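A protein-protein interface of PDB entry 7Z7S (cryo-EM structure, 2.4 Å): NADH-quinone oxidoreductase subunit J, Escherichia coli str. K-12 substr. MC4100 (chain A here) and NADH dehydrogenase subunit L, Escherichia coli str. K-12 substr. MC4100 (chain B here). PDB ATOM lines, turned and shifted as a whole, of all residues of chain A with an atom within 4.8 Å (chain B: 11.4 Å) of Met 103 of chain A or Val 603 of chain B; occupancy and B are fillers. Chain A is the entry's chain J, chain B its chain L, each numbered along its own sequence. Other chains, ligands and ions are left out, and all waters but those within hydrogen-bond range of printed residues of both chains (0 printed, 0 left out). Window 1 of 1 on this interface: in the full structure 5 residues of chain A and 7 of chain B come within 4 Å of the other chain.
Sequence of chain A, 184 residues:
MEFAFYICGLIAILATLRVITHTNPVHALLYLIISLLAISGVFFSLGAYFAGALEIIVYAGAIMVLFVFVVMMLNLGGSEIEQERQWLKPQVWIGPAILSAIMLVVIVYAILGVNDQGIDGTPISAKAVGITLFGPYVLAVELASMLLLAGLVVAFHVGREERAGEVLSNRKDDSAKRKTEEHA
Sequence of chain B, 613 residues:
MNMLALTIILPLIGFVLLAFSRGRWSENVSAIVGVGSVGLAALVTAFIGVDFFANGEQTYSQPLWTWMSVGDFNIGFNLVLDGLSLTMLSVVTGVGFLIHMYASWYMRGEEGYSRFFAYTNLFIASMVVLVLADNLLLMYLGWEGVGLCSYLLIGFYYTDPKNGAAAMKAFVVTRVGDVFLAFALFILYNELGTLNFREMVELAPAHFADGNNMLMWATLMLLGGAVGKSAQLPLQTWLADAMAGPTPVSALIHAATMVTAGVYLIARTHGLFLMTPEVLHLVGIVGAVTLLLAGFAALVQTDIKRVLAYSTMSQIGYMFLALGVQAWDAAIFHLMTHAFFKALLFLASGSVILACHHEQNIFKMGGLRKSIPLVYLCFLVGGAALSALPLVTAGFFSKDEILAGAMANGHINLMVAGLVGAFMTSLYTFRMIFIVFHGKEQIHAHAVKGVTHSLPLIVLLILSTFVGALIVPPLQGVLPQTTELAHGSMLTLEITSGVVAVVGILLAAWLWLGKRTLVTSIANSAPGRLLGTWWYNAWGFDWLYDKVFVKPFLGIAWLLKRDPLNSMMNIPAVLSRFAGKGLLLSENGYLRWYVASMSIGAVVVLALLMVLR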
ATOM      1  N   ILE A  98       1.189  15.948  -1.037  1.00  0.00           N
ATOM      2  CA  ILE A  98       0.458  14.830  -0.441  1.00  0.00           C
ATOM      3  C   ILE A  98       0.823  14.679   1.029  1.00  0.00           C
ATOM      4  O   ILE A  98       0.003  14.218   1.823  1.00  0.00           O
ATOM      5  CB  ILE A  98       0.654  13.483  -1.182  1.00  0.00           C
ATOM      6  CG1 ILE A  98       0.715  13.611  -2.705  1.00  0.00           C
ATOM      7  CG2 ILE A  98      -0.466  12.509  -0.842  1.00  0.00           C
ATOM      8  CD1 ILE A  98       2.089  13.740  -3.262  1.00  0.00           C
ATOM      9  N   LEU A  99       2.041  15.061   1.418  1.00  0.00           N
ATOM     10  CA  LEU A  99       2.426  14.992   2.825  1.00  0.00           C
ATOM     11  C   LEU A  99       1.563  15.918   3.676  1.00  0.00           C
ATOM     12  O   LEU A  99       1.003  15.505   4.702  1.00  0.00           O
ATOM     13  CB  LEU A  99       3.905  15.340   2.968  1.00  0.00           C
ATOM     14  CG  LEU A  99       4.559  15.134   4.331  1.00  0.00           C
ATOM     15  CD1 LEU A  99       4.435  13.689   4.761  1.00  0.00           C
ATOM     16  CD2 LEU A  99       6.011  15.547   4.266  1.00  0.00           C
ATOM     17  N   SER A 100       1.403  17.166   3.229  1.00  0.00           N
ATOM     18  CA  SER A 100       0.515  18.097   3.916  1.00  0.00           C
ATOM     19  C   SER A 100      -0.938  17.650   3.835  1.00  0.00           C
ATOM     20  O   SER A 100      -1.694  17.812   4.799  1.00  0.00           O
ATOM     21  CB  SER A 100       0.672  19.493   3.331  1.00  0.00           C
ATOM     22  OG  SER A 100       1.976  19.995   3.555  1.00  0.00           O
ATOM     23  N   ALA A 101      -1.345  17.081   2.698  1.00  0.00           N
ATOM     24  CA  ALA A 101      -2.723  16.633   2.537  1.00  0.00           C
ATOM     25  C   ALA A 101      -3.059  15.483   3.478  1.00  0.00           C
ATOM     26  O   ALA A 101      -4.139  15.464   4.072  1.00  0.00           O
ATOM     27  CB  ALA A 101      -2.975  16.231   1.085  1.00  0.00           C
ATOM     28  N   ILE A 102      -2.150  14.520   3.640  1.00  0.00           N
ATOM     29  CA  ILE A 102      -2.450  13.407   4.534  1.00  0.00           C
ATOM     30  C   ILE A 102      -2.316  13.829   5.991  1.00  0.00           C
ATOM     31  O   ILE A 102      -3.040  13.308   6.850  1.00  0.00           O
ATOM     32  CB  ILE A 102      -1.593  12.165   4.218  1.00  0.00           C
ATOM     33  CG1 ILE A 102      -0.109  12.408   4.502  1.00  0.00           C
ATOM     34  CG2 ILE A 102      -1.844  11.696   2.785  1.00  0.00           C
ATOM     35  CD1 ILE A 102       0.827  11.450   3.798  1.00  0.00           C
ATOM     36  N   MET A 103      -1.432  14.786   6.305  1.00  0.00           N
ATOM     37  CA  MET A 103      -1.422  15.336   7.656  1.00  0.00           C
ATOM     38  C   MET A 103      -2.739  16.026   7.973  1.00  0.00           C
ATOM     39  O   MET A 103      -3.302  15.841   9.060  1.00  0.00           O
ATOM     40  CB  MET A 103      -0.262  16.309   7.827  1.00  0.00           C
ATOM     41  CG  MET A 103       0.004  16.669   9.271  1.00  0.00           C
ATOM     42  SD  MET A 103       1.249  17.948   9.429  1.00  0.00           S
ATOM     43  CE  MET A 103       2.725  16.956   9.282  1.00  0.00           C
ATOM     44  N   LEU A 104      -3.263  16.795   7.017  1.00  0.00           N
ATOM     45  CA  LEU A 104      -4.555  17.441   7.195  1.00  0.00           C
ATOM     46  C   LEU A 104      -5.674  16.419   7.314  1.00  0.00           C
ATOM     47  O   LEU A 104      -6.599  16.604   8.104  1.00  0.00           O
ATOM     48  CB  LEU A 104      -4.826  18.398   6.039  1.00  0.00           C
ATOM     49  CG  LEU A 104      -6.054  19.287   6.198  1.00  0.00           C
ATOM     50  CD1 LEU A 104      -5.964  20.061   7.494  1.00  0.00           C
ATOM     51  CD2 LEU A 104      -6.174  20.222   5.019  1.00  0.00           C
ATOM     52  N   VAL A 105      -5.599  15.331   6.545  1.00  0.00           N
ATOM     53  CA  VAL A 105      -6.632  14.298   6.592  1.00  0.00           C
ATOM     54  C   VAL A 105      -6.655  13.621   7.959  1.00  0.00           C
ATOM     55  O   VAL A 105      -7.725  13.424   8.547  1.00  0.00           O
ATOM     56  CB  VAL A 105      -6.421  13.288   5.447  1.00  0.00           C
ATOM     57  CG1 VAL A 105      -7.043  11.938   5.769  1.00  0.00           C
ATOM     58  CG2 VAL A 105      -7.003  13.829   4.158  1.00  0.00           C
ATOM     59  N   VAL A 106      -5.480  13.288   8.499  1.00  0.00           N
ATOM     60  CA  VAL A 106      -5.424  12.643   9.810  1.00  0.00           C
ATOM     61  C   VAL A 106      -5.888  13.598  10.910  1.00  0.00           C
ATOM     62  O   VAL A 106      -6.662  13.211  11.799  1.00  0.00           O
ATOM     63  CB  VAL A 106      -4.008  12.103  10.083  1.00  0.00           C
ATOM     64  CG1 VAL A 106      -3.927  11.532  11.476  1.00  0.00           C
ATOM     65  CG2 VAL A 106      -3.648  11.035   9.077  1.00  0.00           C
ATOM     66  N   ILE A 107      -5.447  14.860  10.858  1.00  0.00           N
ATOM     67  CA  ILE A 107      -5.849  15.830  11.875  1.00  0.00           C
ATOM     68  C   ILE A 107      -7.351  16.101  11.803  1.00  0.00           C
ATOM     69  O   ILE A 107      -8.024  16.203  12.834  1.00  0.00           O
ATOM     70  CB  ILE A 107      -5.018  17.120  11.734  1.00  0.00           C
ATOM     71  CG1 ILE A 107      -3.564  16.856  12.108  1.00  0.00           C
ATOM     72  CG2 ILE A 107      -5.543  18.212  12.633  1.00  0.00           C
ATOM     73  CD1 ILE A 107      -2.620  17.969  11.711  1.00  0.00           C
ATOM     74  N   TYR B 594      15.142  18.381   6.539  1.00  0.00           N
ATOM     75  CA  TYR B 594      14.918  18.154   7.964  1.00  0.00           C
ATOM     76  C   TYR B 594      13.490  18.524   8.362  1.00  0.00           C
ATOM     77  O   TYR B 594      12.846  17.807   9.140  1.00  0.00           O
ATOM     78  CB  TYR B 594      15.928  18.947   8.787  1.00  0.00           C
ATOM     79  CG  TYR B 594      17.370  18.496   8.662  1.00  0.00           C
ATOM     80  CD1 TYR B 594      17.711  17.325   7.993  1.00  0.00           C
ATOM     81  CD2 TYR B 594      18.391  19.245   9.220  1.00  0.00           C
ATOM     82  CE1 TYR B 594      19.023  16.926   7.881  1.00  0.00           C
ATOM     83  CE2 TYR B 594      19.702  18.847   9.117  1.00  0.00           C
ATOM     84  CZ  TYR B 594      20.011  17.690   8.447  1.00  0.00           C
ATOM     85  OH  TYR B 594      21.319  17.295   8.345  1.00  0.00           O
ATOM     86  N   VAL B 595      12.971  19.626   7.811  1.00  0.00           N
ATOM     87  CA  VAL B 595      11.575  19.993   8.036  1.00  0.00           C
ATOM     88  C   VAL B 595      10.637  18.949   7.438  1.00  0.00           C
ATOM     89  O   VAL B 595       9.623  18.578   8.046  1.00  0.00           O
ATOM     90  CB  VAL B 595      11.291  21.395   7.465  1.00  0.00           C
ATOM     91  CG1 VAL B 595       9.873  21.802   7.762  1.00  0.00           C
ATOM     92  CG2 VAL B 595      12.246  22.408   8.041  1.00  0.00           C
ATOM     93  N   ALA B 596      10.962  18.457   6.241  1.00  0.00           N
ATOM     94  CA  ALA B 596      10.141  17.433   5.606  1.00  0.00           C
ATOM     95  C   ALA B 596      10.139  16.140   6.412  1.00  0.00           C
ATOM     96  O   ALA B 596       9.115  15.459   6.498  1.00  0.00           O
ATOM     97  CB  ALA B 596      10.636  17.177   4.184  1.00  0.00           C
ATOM     98  N   SER B 597      11.276  15.794   7.016  1.00  0.00           N
ATOM     99  CA  SER B 597      11.347  14.593   7.838  1.00  0.00           C
ATOM    100  C   SER B 597      10.564  14.763   9.131  1.00  0.00           C
ATOM    101  O   SER B 597       9.961  13.805   9.624  1.00  0.00           O
ATOM    102  CB  SER B 597      12.799  14.242   8.136  1.00  0.00           C
ATOM    103  OG  SER B 597      13.300  15.045   9.185  1.00  0.00           O
ATOM    104  N   MET B 598      10.559  15.975   9.694  1.00  0.00           N
ATOM    105  CA  MET B 598       9.703  16.241  10.849  1.00  0.00           C
ATOM    106  C   MET B 598       8.226  16.101  10.489  1.00  0.00           C
ATOM    107  O   MET B 598       7.442  15.540  11.263  1.00  0.00           O
ATOM    108  CB  MET B 598       9.992  17.629  11.414  1.00  0.00           C
ATOM    109  CG  MET B 598      11.007  17.634  12.541  1.00  0.00           C
ATOM    110  SD  MET B 598      11.284  19.274  13.238  1.00  0.00           S
ATOM    111  CE  MET B 598       9.603  19.874  13.369  1.00  0.00           C
ATOM    112  N   SER B 599       7.834  16.585   9.308  1.00  0.00           N
ATOM    113  CA  SER B 599       6.452  16.420   8.853  1.00  0.00           C
ATOM    114  C   SER B 599       6.108  14.954   8.599  1.00  0.00           C
ATOM    115  O   SER B 599       4.995  14.507   8.906  1.00  0.00           O
ATOM    116  CB  SER B 599       6.216  17.246   7.592  1.00  0.00           C
ATOM    117  OG  SER B 599       6.817  18.519   7.699  1.00  0.00           O
ATOM    118  N   ILE B 600       7.050  14.197   8.029  1.00  0.00           N
ATOM    119  CA  ILE B 600       6.850  12.770   7.788  1.00  0.00           C
ATOM    120  C   ILE B 600       6.670  12.028   9.105  1.00  0.00           C
ATOM    121  O   ILE B 600       5.772  11.186   9.246  1.00  0.00           O
ATOM    122  CB  ILE B 600       8.030  12.203   6.975  1.00  0.00           C
ATOM    123  CG1 ILE B 600       7.917  12.597   5.504  1.00  0.00           C
ATOM    124  CG2 ILE B 600       8.114  10.689   7.092  1.00  0.00           C
ATOM    125  CD1 ILE B 600       9.222  12.489   4.752  1.00  0.00           C
ATOM    126  N   GLY B 601       7.514  12.338  10.091  1.00  0.00           N
ATOM    127  CA  GLY B 601       7.379  11.719  11.397  1.00  0.00           C
ATOM    128  C   GLY B 601       6.089  12.096  12.095  1.00  0.00           C
ATOM    129  O   GLY B 601       5.501  11.279  12.804  1.00  0.00           O
ATOM    130  N   ALA B 602       5.631  13.336  11.903  1.00  0.00           N
ATOM    131  CA  ALA B 602       4.340  13.738  12.448  1.00  0.00           C
ATOM    132  C   ALA B 602       3.206  12.937  11.829  1.00  0.00           C
ATOM    133  O   ALA B 602       2.303  12.481  12.538  1.00  0.00           O
ATOM    134  CB  ALA B 602       4.124  15.233  12.233  1.00  0.00           C
ATOM    135  N   VAL B 603       3.250  12.739  10.510  1.00  0.00           N
ATOM    136  CA  VAL B 603       2.230  11.944   9.829  1.00  0.00           C
ATOM    137  C   VAL B 603       2.247  10.506  10.333  1.00  0.00           C
ATOM    138  O   VAL B 603       1.194   9.916  10.606  1.00  0.00           O
ATOM    139  CB  VAL B 603       2.434  12.018   8.303  1.00  0.00           C
ATOM    140  CG1 VAL B 603       1.640  10.940   7.590  1.00  0.00           C
ATOM    141  CG2 VAL B 603       2.039  13.380   7.784  1.00  0.00           C
ATOM    142  N   VAL B 604       3.443   9.933  10.493  1.00  0.00           N
ATOM    143  CA  VAL B 604       3.567   8.548  10.945  1.00  0.00           C
ATOM    144  C   VAL B 604       3.056   8.392  12.374  1.00  0.00           C
ATOM    145  O   VAL B 604       2.293   7.464  12.671  1.00  0.00           O
ATOM    146  CB  VAL B 604       5.024   8.077  10.803  1.00  0.00           C
ATOM    147  CG1 VAL B 604       5.255   6.790  11.570  1.00  0.00           C
ATOM    148  CG2 VAL B 604       5.371   7.887   9.341  1.00  0.00           C
ATOM    149  N   VAL B 605       3.442   9.309  13.269  1.00  0.00           N
ATOM    150  CA  VAL B 605       3.008   9.252  14.663  1.00  0.00           C
ATOM    151  C   VAL B 605       1.496   9.406  14.764  1.00  0.00           C
ATOM    152  O   VAL B 605       0.829   8.655  15.489  1.00  0.00           O
ATOM    153  CB  VAL B 605       3.748  10.325  15.488  1.00  0.00           C
ATOM    154  CG1 VAL B 605       3.005  10.644  16.776  1.00  0.00           C
ATOM    155  CG2 VAL B 605       5.158   9.878  15.793  1.00  0.00           C
ATOM    156  N   LEU B 606       0.927  10.358  14.020  1.00  0.00           N
ATOM    157  CA  LEU B 606      -0.511  10.588  14.085  1.00  0.00           C
ATOM    158  C   LEU B 606      -1.297   9.418  13.506  1.00  0.00           C
ATOM    159  O   LEU B 606      -2.328   9.027  14.063  1.00  0.00           O
ATOM    160  CB  LEU B 606      -0.861  11.883  13.359  1.00  0.00           C
ATOM    161  CG  LEU B 606      -0.490  13.195  14.050  1.00  0.00           C
ATOM    162  CD1 LEU B 606      -0.926  14.363  13.195  1.00  0.00           C
ATOM    163  CD2 LEU B 606      -1.104  13.271  15.424  1.00  0.00           C
ATOM    164  N   ALA B 607      -0.825   8.837  12.399  1.00  0.00           N
ATOM    165  CA  ALA B 607      -1.504   7.680  11.825  1.00  0.00           C
ATOM    166  C   ALA B 607      -1.424   6.473  12.749  1.00  0.00           C
ATOM    167  O   ALA B 607      -2.400   5.724  12.883  1.00  0.00           O
ATOM    168  CB  ALA B 607      -0.908   7.348  10.460  1.00  0.00           C
ATOM    169  N   LEU B 608      -0.276   6.276  13.403  1.00  0.00           N
ATOM    170  CA  LEU B 608      -0.140   5.176  14.350  1.00  0.00           C
ATOM    171  C   LEU B 608      -1.039   5.371  15.561  1.00  0.00           C
ATOM    172  O   LEU B 608      -1.596   4.404  16.087  1.00  0.00           O
ATOM    173  CB  LEU B 608       1.315   5.034  14.781  1.00  0.00           C
ATOM    174  CG  LEU B 608       2.204   4.247  13.825  1.00  0.00           C
ATOM    175  CD1 LEU B 608       3.609   4.157  14.374  1.00  0.00           C
ATOM    176  CD2 LEU B 608       1.625   2.867  13.600  1.00  0.00           C
ATOM    177  N   LEU B 609      -1.191   6.610  16.022  1.00  0.00           N
ATOM    178  CA  LEU B 609      -2.108   6.862  17.126  1.00  0.00           C
ATOM    179  C   LEU B 609      -3.560   6.683  16.706  1.00  0.00           C
ATOM    180  O   LEU B 609      -4.392   6.268  17.519  1.00  0.00           O
ATOM    181  CB  LEU B 609      -1.884   8.262  17.684  1.00  0.00           C
ATOM    182  CG  LEU B 609      -0.743   8.332  18.688  1.00  0.00           C
ATOM    183  CD1 LEU B 609      -0.339   9.761  18.926  1.00  0.00           C
ATOM    184  CD2 LEU B 609      -1.170   7.680  19.974  1.00  0.00           C
ATOM    185  N   MET B 610      -3.885   6.990  15.450  1.00  0.00           N
ATOM    186  CA  MET B 610      -5.258   6.831  14.989  1.00  0.00           C
ATOM    187  C   MET B 610      -5.623   5.364  14.802  1.00  0.00           C
ATOM    188  O   MET B 610      -6.755   4.963  15.096  1.00  0.00           O
ATOM    189  CB  MET B 610      -5.472   7.609  13.692  1.00  0.00           C
ATOM    190  CG  MET B 610      -5.589   9.114  13.884  1.00  0.00           C
ATOM    191  SD  MET B 610      -6.723   9.586  15.203  1.00  0.00           S
ATOM    192  CE  MET B 610      -5.581  10.265  16.403  1.00  0.00           C
ATOM    193  N   VAL B 611      -4.691   4.544  14.310  1.00  0.00           N
ATOM    194  CA  VAL B 611      -5.021   3.137  14.087  1.00  0.00           C
ATOM    195  C   VAL B 611      -5.016   2.324  15.376  1.00  0.00           C
ATOM    196  O   VAL B 611      -5.577   1.222  15.403  1.00  0.00           O
ATOM    197  CB  VAL B 611      -4.083   2.486  13.059  1.00  0.00           C
ATOM    198  CG1 VAL B 611      -4.197   3.188  11.721  1.00  0.00           C
ATOM    199  CG2 VAL B 611      -2.656   2.492  13.550  1.00  0.00           C
ATOM    200  N   LEU B 612      -4.407   2.826  16.445  1.00  0.00           N
ATOM    201  CA  LEU B 612      -4.468   2.166  17.745  1.00  0.00           C
ATOM    202  C   LEU B 612      -5.092   3.082  18.792  1.00  0.00           C
ATOM    203  O   LEU B 612      -6.193   2.831  19.275  1.00  0.00           O
ATOM    204  CB  LEU B 612      -3.076   1.724  18.202  1.00  0.00           C
ATOM    205  CG  LEU B 612      -2.039   1.357  17.142  1.00  0.00           C
ATOM    206  CD1 LEU B 612      -0.680   1.167  17.775  1.00  0.00           C
ATOM    207  CD2 LEU B 612      -2.460   0.086  16.430  1.00  0.00           C
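The side-chain hydroxyl (OG) of Ser 599 of chain B sits at hydrogen-bond distance from the backbone carbonyl oxygen (O) of Val 595 of chain B, 2.8 Å away.
Leu 99 of chain A touches Ala 596 of chain B (CD2 to O, 3.8 Å). Leu 99 of chain A touches Ser 599 of chain B. Leu 99 of chain A touches Ile 600 of chain B. Val 603 of chain B touches Leu 99 of chain A. Val 603 of chain B touches Ile 102 of chain A (CG1 to CG1, 3.8 Å). Met 103 of chain A touches Ser 599 of chain B. Met 103 of chain A touches Val 603 of chain B (CB to CG2, 3.7 Å). Val 106 of chain A touches Leu 606 of chain B (CG1 to CB, 3.6 Å). Val 106 of chain A touches Met 610 of chain B. Ile 107 of chain A touches Leu 606 of chain B.
Leu 99 of chain A touches just these residues of chain B: Ala 596 (3.8 Å), Ser 599 (3.7 Å), Ile 600 (3.7 Å) and Val 603 (3.9 Å). Ser 100 of chain A touches none of the printed residues of chain B. No residue of chain B comes within 4 Å of Ala 101 of chain A. Printed residues of chain B within 4 Å of Ile 102 of chain A: Val 603. Of chain B, only Ser 599 (3.4 Å), Ala 602 (3.7 Å) and Val 603 (3.7 Å) come within 4 Å of Met 103 of chain A. Leu 104 of chain A touches none of the printed residues of chain B. Printed residues of chain A within 4 Å of Ala 596 of chain B: Leu 99 (3.8 Å). Of the printed residues of chain A, Ser 599 of chain B touches Leu 99 and Met 103. Printed residues of chain A within 4 Å of Ile 600 of chain B: Leu 99 (3.7 Å). Printed residues of chain A within 4 Å of Ala 602 of chain B: Met 103 (3.7 Å). Of chain A, only Leu 99 (3.9 Å), Ile 102 (3.8 Å) and Met 103 (3.7 Å) come within 4 Å of Val 603 of chain B. Printed residues of chain A within 4 Å of Met 610 of chain B: Val 106 (3.8 Å). The nearest residue of chain B that does not touch Met 103 of chain A is Leu 606 of chain B (4.6 Å). The nearest printed residue of chain A that does not touch Leu 606 of chain B is Met 103 of chain A (4.6 Å).
Printed residues of chain B that touch a printed residue of chain A: Ala 596, Ser 599, Ile 600, Ala 602, Val 603, Leu 606 and Met 610. Along chain B the printed residues that touch a printed residue of chain A span positions 596 to 610. Of the 10 printed residues of chain A, 5 touch a printed residue of chain B. Hydrophobic or aromatic side chains of chain A within 4 Å of the printed part of chain B: Leu 99, Ile 102, Met 103, Val 106 and Ile 107. Among the printed residues, 11 pairs touch across the chains. Among the printed residues, no Asp or Glu carboxylate lies within 4 Å of a Lys or Arg side-chain nitrogen of the other chain.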
